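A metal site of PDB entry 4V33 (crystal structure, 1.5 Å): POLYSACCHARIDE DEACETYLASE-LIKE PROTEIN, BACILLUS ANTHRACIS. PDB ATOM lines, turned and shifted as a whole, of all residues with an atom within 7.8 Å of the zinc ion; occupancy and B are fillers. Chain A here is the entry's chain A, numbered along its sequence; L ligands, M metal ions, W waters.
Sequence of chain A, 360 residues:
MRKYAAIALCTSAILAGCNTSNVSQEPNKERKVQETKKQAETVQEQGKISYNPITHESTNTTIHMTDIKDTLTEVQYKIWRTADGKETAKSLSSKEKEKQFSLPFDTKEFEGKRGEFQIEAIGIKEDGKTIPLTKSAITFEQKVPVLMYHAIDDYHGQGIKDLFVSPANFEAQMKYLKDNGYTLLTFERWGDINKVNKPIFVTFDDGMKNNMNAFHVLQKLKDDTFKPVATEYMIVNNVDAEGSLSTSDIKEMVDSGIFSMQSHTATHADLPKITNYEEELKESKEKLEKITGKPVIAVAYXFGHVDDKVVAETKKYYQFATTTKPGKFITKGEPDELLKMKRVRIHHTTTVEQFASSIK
NE2 of His 268 sits close to OA of PXU 302, at 3.2 Å. The backbone carbonyl oxygen (O) of Asp 206 is in hydrogen-bond range of the backbone NH (N) of Ile 235 (3.1 Å). The backbone NH of Asp 206 sits at hydrogen-bond distance from the backbone carbonyl oxygen of Tyr 233 (2.8 Å). OA of PXU 302 lies close to a ring nitrogen (NE2) of His 264. The backbone carbonyl oxygen (O) of Ala 300 is in hydrogen-bond range of a ring nitrogen (ND1) of His 264 (3.0 Å). OD2 of Asp 205 lies within salt-bridge range of NH2 of Arg 343 (2.8 Å). N of Asp 205 lies within hydrogen-bond range of O of Tyr 149 (2.9 Å).
Asp 205 touches the zinc ion (CB to ZN, 3.98 Å). PXU 302 touches the zinc ion (OA to ZN, 3.6 Å). The nearest printed residue that does not touch the zinc ion is His 150 (4.4 Å).
The zinc ion is bound by water W1, at 2.0 Å. The zinc ion is bound by a ring nitrogen (NE2) of His 268, at 2.1 Å. The zinc ion is bound by OD1 of Asp 206 (2.1 Å). The zinc ion is bound by NE2 of His 264 (2.2 Å). The zinc ion is bound by O1 of the ligand. Slightly farther from the zinc ion lies O2 of the ligand (2.7 Å).
Water W1 lies within hydrogen-bond range of OD2 of Asp 206 (2.9 Å) and NE2 of His 150 (3.5 Å).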
ATOM      1  N   MET A 148       1.325  28.782 -11.281  1.00  0.00           N
ATOM      2  CA  MET A 148       0.413  28.232 -12.278  1.00  0.00           C
ATOM      3  C   MET A 148      -0.566  29.305 -12.773  1.00  0.00           C
ATOM      4  O   MET A 148      -1.417  29.776 -12.010  1.00  0.00           O
ATOM      5  CB  MET A 148      -0.370  27.067 -11.707  1.00  0.00           C
ATOM      6  CG  MET A 148      -1.408  26.505 -12.687  1.00  0.00           C
ATOM      7  SD  MET A 148      -2.309  25.095 -12.045  1.00  0.00           S
ATOM      8  CE  MET A 148      -2.978  25.809 -10.551  1.00  0.00           C
ATOM      9  N   TYR A 149      -0.401  29.673 -14.040  1.00  0.00           N
ATOM     10  CA  TYR A 149      -1.340  30.530 -14.750  1.00  0.00           C
ATOM     11  C   TYR A 149      -2.117  29.738 -15.790  1.00  0.00           C
ATOM     12  O   TYR A 149      -1.706  28.637 -16.180  1.00  0.00           O
ATOM     13  CB  TYR A 149      -0.590  31.639 -15.484  1.00  0.00           C
ATOM     14  CG  TYR A 149       0.052  32.670 -14.591  1.00  0.00           C
ATOM     15  CD1 TYR A 149      -0.683  33.778 -14.149  1.00  0.00           C
ATOM     16  CD2 TYR A 149       1.374  32.563 -14.202  1.00  0.00           C
ATOM     17  CE1 TYR A 149      -0.116  34.735 -13.349  1.00  0.00           C
ATOM     18  CE2 TYR A 149       1.955  33.525 -13.392  1.00  0.00           C
ATOM     19  CZ  TYR A 149       1.212  34.616 -12.971  1.00  0.00           C
ATOM     20  OH  TYR A 149       1.807  35.561 -12.171  1.00  0.00           O
ATOM     21  N   HIS A 150      -3.251  30.277 -16.223  1.00  0.00           N
ATOM     22  CA  HIS A 150      -4.009  29.729 -17.337  1.00  0.00           C
ATOM     23  C   HIS A 150      -4.168  30.765 -18.434  1.00  0.00           C
ATOM     24  O   HIS A 150      -3.282  30.925 -19.269  1.00  0.00           O
ATOM     25  CB  HIS A 150      -5.353  29.181 -16.853  1.00  0.00           C
ATOM     26  CG  HIS A 150      -5.231  27.871 -16.144  1.00  0.00           C
ATOM     27  ND1 HIS A 150      -4.779  27.769 -14.845  1.00  0.00           N
ATOM     28  CD2 HIS A 150      -5.455  26.610 -16.573  1.00  0.00           C
ATOM     29  CE1 HIS A 150      -4.771  26.488 -14.488  1.00  0.00           C
ATOM     30  NE2 HIS A 150      -5.157  25.767 -15.527  1.00  0.00           N
ATOM     31  N   LEU A 163      -9.835  31.622 -13.933  1.00  0.00           N
ATOM     32  CA  LEU A 163      -8.669  31.223 -14.706  1.00  0.00           C
ATOM     33  C   LEU A 163      -8.125  32.328 -15.605  1.00  0.00           C
ATOM     34  O   LEU A 163      -7.183  32.091 -16.369  1.00  0.00           O
ATOM     35  CB  LEU A 163      -8.987  29.985 -15.547  1.00  0.00           C
ATOM     36  CG  LEU A 163      -9.383  28.742 -14.739  1.00  0.00           C
ATOM     37  CD1 LEU A 163      -9.685  27.588 -15.687  1.00  0.00           C
ATOM     38  CD2 LEU A 163      -8.298  28.379 -13.772  1.00  0.00           C
ATOM     39  N   PHE A 204       2.397  28.086 -17.417  1.00  0.00           N
ATOM     40  CA  PHE A 204       1.082  28.305 -18.003  1.00  0.00           C
ATOM     41  C   PHE A 204       0.517  26.986 -18.452  1.00  0.00           C
ATOM     42  O   PHE A 204       1.227  26.167 -19.057  1.00  0.00           O
ATOM     43  CB  PHE A 204       1.199  29.194 -19.248  1.00  0.00           C
ATOM     44  CG  PHE A 204       1.762  30.554 -18.958  1.00  0.00           C
ATOM     45  CD1 PHE A 204       3.136  30.757 -18.990  1.00  0.00           C
ATOM     46  CD2 PHE A 204       0.934  31.620 -18.660  1.00  0.00           C
ATOM     47  CE1 PHE A 204       3.683  32.004 -18.724  1.00  0.00           C
ATOM     48  CE2 PHE A 204       1.476  32.880 -18.384  1.00  0.00           C
ATOM     49  CZ  PHE A 204       2.846  33.074 -18.426  1.00  0.00           C
ATOM     50  N   ASP A 205      -0.764  26.777 -18.178  1.00  0.00           N
ATOM     51  CA  ASP A 205      -1.434  25.545 -18.586  1.00  0.00           C
ATOM     52  C   ASP A 205      -2.362  25.760 -19.764  1.00  0.00           C
ATOM     53  O   ASP A 205      -3.228  26.656 -19.721  1.00  0.00           O
ATOM     54  CB  ASP A 205      -2.251  24.951 -17.431  1.00  0.00           C
ATOM     55  CG  ASP A 205      -1.379  24.274 -16.387  1.00  0.00           C
ATOM     56  OD1 ASP A 205      -0.150  24.420 -16.424  1.00  0.00           O
ATOM     57  OD2 ASP A 205      -1.941  23.580 -15.518  1.00  0.00           O
ATOM     58  N   ASP A 206      -2.155  24.923 -20.781  1.00  0.00           N
ATOM     59  CA  ASP A 206      -3.095  24.585 -21.883  1.00  0.00           C
ATOM     60  C   ASP A 206      -2.644  25.008 -23.282  1.00  0.00           C
ATOM     61  O   ASP A 206      -2.958  24.330 -24.258  1.00  0.00           O
ATOM     62  CB  ASP A 206      -4.546  25.041 -21.666  1.00  0.00           C
ATOM     63  CG  ASP A 206      -5.205  24.409 -20.447  1.00  0.00           C
ATOM     64  OD1 ASP A 206      -4.609  23.538 -19.756  1.00  0.00           O
ATOM     65  OD2 ASP A 206      -6.366  24.804 -20.194  1.00  0.00           O
ATOM     66  N   GLY A 207      -1.913  26.113 -23.386  1.00  0.00           N
ATOM     67  CA  GLY A 207      -1.523  26.625 -24.684  1.00  0.00           C
ATOM     68  C   GLY A 207      -2.592  27.460 -25.348  1.00  0.00           C
ATOM     69  O   GLY A 207      -2.783  27.412 -26.554  1.00  0.00           O
ATOM     70  N   MET A 208      -3.319  28.246 -24.544  1.00  0.00           N
ATOM     71  CA  MET A 208      -4.272  29.201 -25.092  1.00  0.00           C
ATOM     72  C   MET A 208      -3.561  30.265 -25.927  1.00  0.00           C
ATOM     73  O   MET A 208      -2.451  30.700 -25.589  1.00  0.00           O
ATOM     74  CB  MET A 208      -5.067  29.864 -23.972  1.00  0.00           C
ATOM     75  CG  MET A 208      -6.018  28.920 -23.289  1.00  0.00           C
ATOM     76  SD  MET A 208      -6.895  29.751 -21.938  1.00  0.00           S
ATOM     77  CE  MET A 208      -6.095  28.972 -20.538  1.00  0.00           C
ATOM     78  N   TYR A 233       2.712  24.587 -20.834  1.00  0.00           N
ATOM     79  CA  TYR A 233       2.308  23.197 -20.961  1.00  0.00           C
ATOM     80  C   TYR A 233       1.193  23.107 -22.000  1.00  0.00           C
ATOM     81  O   TYR A 233       0.050  23.471 -21.738  1.00  0.00           O
ATOM     82  CB  TYR A 233       1.802  22.669 -19.626  1.00  0.00           C
ATOM     83  CG  TYR A 233       2.809  22.562 -18.484  1.00  0.00           C
ATOM     84  CD1 TYR A 233       3.787  21.573 -18.487  1.00  0.00           C
ATOM     85  CD2 TYR A 233       2.726  23.408 -17.383  1.00  0.00           C
ATOM     86  CE1 TYR A 233       4.677  21.444 -17.428  1.00  0.00           C
ATOM     87  CE2 TYR A 233       3.606  23.283 -16.315  1.00  0.00           C
ATOM     88  CZ  TYR A 233       4.562  22.293 -16.338  1.00  0.00           C
ATOM     89  OH  TYR A 233       5.417  22.157 -15.281  1.00  0.00           O
ATOM     90  N   ILE A 235      -1.516  21.583 -24.617  1.00  0.00           N
ATOM     91  CA  ILE A 235      -2.376  20.465 -25.007  1.00  0.00           C
ATOM     92  C   ILE A 235      -2.014  20.176 -26.457  1.00  0.00           C
ATOM     93  O   ILE A 235      -2.340  20.960 -27.344  1.00  0.00           O
ATOM     94  CB  ILE A 235      -3.868  20.799 -24.863  1.00  0.00           C
ATOM     95  CG1 ILE A 235      -4.204  21.021 -23.385  1.00  0.00           C
ATOM     96  CG2 ILE A 235      -4.740  19.649 -25.415  1.00  0.00           C
ATOM     97  CD1 ILE A 235      -5.565  21.710 -23.169  1.00  0.00           C
ATOM     98  N   HIS A 264       1.087  19.062 -21.939  1.00  0.00           N
ATOM     99  CA  HIS A 264      -0.113  18.983 -21.090  1.00  0.00           C
ATOM    100  C   HIS A 264      -0.955  17.805 -21.541  1.00  0.00           C
ATOM    101  O   HIS A 264      -2.178  17.828 -21.429  1.00  0.00           O
ATOM    102  CB  HIS A 264      -0.922  20.284 -21.165  1.00  0.00           C
ATOM    103  CG  HIS A 264      -1.741  20.593 -19.935  1.00  0.00           C
ATOM    104  ND1 HIS A 264      -1.616  19.907 -18.750  1.00  0.00           N
ATOM    105  CD2 HIS A 264      -2.685  21.538 -19.723  1.00  0.00           C
ATOM    106  CE1 HIS A 264      -2.468  20.406 -17.856  1.00  0.00           C
ATOM    107  NE2 HIS A 264      -3.132  21.400 -18.426  1.00  0.00           N
ATOM    108  N   HIS A 268      -5.594  16.637 -23.013  1.00  0.00           N
ATOM    109  CA  HIS A 268      -5.932  17.127 -21.667  1.00  0.00           C
ATOM    110  C   HIS A 268      -6.714  16.021 -20.945  1.00  0.00           C
ATOM    111  O   HIS A 268      -7.796  16.230 -20.405  1.00  0.00           O
ATOM    112  CB  HIS A 268      -6.725  18.442 -21.722  1.00  0.00           C
ATOM    113  CG  HIS A 268      -6.689  19.241 -20.459  1.00  0.00           C
ATOM    114  ND1 HIS A 268      -7.759  19.312 -19.592  1.00  0.00           N
ATOM    115  CD2 HIS A 268      -5.738  20.043 -19.935  1.00  0.00           C
ATOM    116  CE1 HIS A 268      -7.460  20.105 -18.583  1.00  0.00           C
ATOM    117  NE2 HIS A 268      -6.241  20.577 -18.772  1.00  0.00           N
ATOM    118  N   ALA A 300       2.364  18.574 -17.149  1.00  0.00           N
ATOM    119  CA  ALA A 300       1.469  18.954 -16.070  1.00  0.00           C
ATOM    120  C   ALA A 300       0.275  18.033 -16.112  1.00  0.00           C
ATOM    121  O   ALA A 300      -0.266  17.784 -17.192  1.00  0.00           O
ATOM    122  CB  ALA A 300       1.025  20.417 -16.222  1.00  0.00           C
ATOM    123  N   TYR A 301      -0.151  17.510 -14.965  1.00  0.00           N
ATOM    124  CA  TYR A 301      -1.297  16.599 -14.937  1.00  0.00           C
ATOM    125  C   TYR A 301      -2.617  17.371 -15.098  1.00  0.00           C
ATOM    126  O   TYR A 301      -2.932  18.252 -14.302  1.00  0.00           O
ATOM    127  CB  TYR A 301      -1.356  15.845 -13.607  1.00  0.00           C
ATOM    128  CG  TYR A 301      -0.145  15.004 -13.270  1.00  0.00           C
ATOM    129  CD1 TYR A 301       0.234  13.943 -14.080  1.00  0.00           C
ATOM    130  CD2 TYR A 301       0.605  15.259 -12.125  1.00  0.00           C
ATOM    131  CE1 TYR A 301       1.327  13.154 -13.764  1.00  0.00           C
ATOM    132  CE2 TYR A 301       1.707  14.465 -11.800  1.00  0.00           C
ATOM    133  CZ  TYR A 301       2.059  13.417 -12.629  1.00  0.00           C
ATOM    134  OH  TYR A 301       3.149  12.619 -12.334  1.00  0.00           O
ATOM    135  N   PXU A 302      -3.409  16.998 -16.097  1.00  0.00           N
ATOM    136  CA  PXU A 302      -4.612  17.613 -16.310  1.00  0.00           C
ATOM    137  OA  PXU A 302      -4.572  19.033 -16.552  1.00  0.00           O
ATOM    138  CB  PXU A 302      -5.230  16.827 -17.606  1.00  0.00           C
ATOM    139  CG  PXU A 302      -4.193  16.558 -18.339  1.00  0.00           C
ATOM    140  CD  PXU A 302      -3.115  16.131 -17.324  1.00  0.00           C
ATOM    141  C   PXU A 302      -5.520  17.513 -15.073  1.00  0.00           C
ATOM    142  O   PXU A 302      -5.609  16.418 -14.474  1.00  0.00           O
ATOM    143  N   PHE A 303      -6.155  18.624 -14.689  1.00  0.00           N
ATOM    144  CA  PHE A 303      -7.049  18.684 -13.518  1.00  0.00           C
ATOM    145  C   PHE A 303      -6.327  18.476 -12.185  1.00  0.00           C
ATOM    146  O   PHE A 303      -6.956  18.437 -11.131  1.00  0.00           O
ATOM    147  CB  PHE A 303      -8.238  17.720 -13.632  1.00  0.00           C
ATOM    148  CG  PHE A 303      -8.869  17.683 -14.998  1.00  0.00           C
ATOM    149  CD1 PHE A 303      -9.674  18.733 -15.420  1.00  0.00           C
ATOM    150  CD2 PHE A 303      -8.658  16.610 -15.852  1.00  0.00           C
ATOM    151  CE1 PHE A 303     -10.259  18.705 -16.676  1.00  0.00           C
ATOM    152  CE2 PHE A 303      -9.234  16.578 -17.108  1.00  0.00           C
ATOM    153  CZ  PHE A 303     -10.026  17.632 -17.519  1.00  0.00           C
ATOM    154  N   GLY A 304      -5.001  18.341 -12.247  1.00  0.00           N
ATOM    155  CA  GLY A 304      -4.230  17.965 -11.078  1.00  0.00           C
ATOM    156  C   GLY A 304      -4.479  16.520 -10.662  1.00  0.00           C
ATOM    157  O   GLY A 304      -4.122  16.118  -9.543  1.00  0.00           O
ATOM    158  N   THR A 324      -1.650  20.132  -9.028  1.00  0.00           N
ATOM    159  CA  THR A 324      -2.260  21.381  -8.570  1.00  0.00           C
ATOM    160  C   THR A 324      -2.347  21.450  -7.049  1.00  0.00           C
ATOM    161  O   THR A 324      -3.083  22.283  -6.514  1.00  0.00           O
ATOM    162  CB  THR A 324      -3.655  21.615  -9.197  1.00  0.00           C
ATOM    163  OG1 THR A 324      -4.536  20.544  -8.846  1.00  0.00           O
ATOM    164  CG2 THR A 324      -3.542  21.731 -10.712  1.00  0.00           C
ATOM    165  N   ARG A 343       2.264  23.322  -6.910  1.00  0.00           N
ATOM    166  CA  ARG A 343       2.255  24.615  -7.576  1.00  0.00           C
ATOM    167  C   ARG A 343       1.469  25.667  -6.807  1.00  0.00           C
ATOM    168  O   ARG A 343       0.584  25.356  -6.005  1.00  0.00           O
ATOM    169  CB  ARG A 343       1.733  24.501  -9.013  1.00  0.00           C
ATOM    170  CG  ARG A 343       2.659  23.719  -9.932  1.00  0.00           C
ATOM    171  CD  ARG A 343       2.324  23.961 -11.384  1.00  0.00           C
ATOM    172  NE  ARG A 343       1.168  23.191 -11.822  1.00  0.00           N
ATOM    173  CZ  ARG A 343       0.609  23.324 -13.023  1.00  0.00           C
ATOM    174  NH1 ARG A 343       1.101  24.211 -13.878  1.00  0.00           N
ATOM    175  NH2 ARG A 343      -0.429  22.553 -13.358  1.00  0.00           N
HETATM  176  C1  LIG L   1      -4.875  22.018 -15.319  1.00  0.00           C
HETATM  177  O1  LIG L   1      -4.483  23.007 -15.984  1.00  0.00           O
HETATM  178  O2  LIG L   1      -5.961  21.464 -15.640  1.00  0.00           O
HETATM  179  C2  LIG L   1      -4.069  21.497 -14.163  1.00  0.00           C
HETATM  180 ZN    ZN M   1      -5.090  22.247 -18.120  1.00  0.00          ZN
HETATM  181  O   HOH W   1      -6.661  23.464 -17.645  1.00  0.00           O
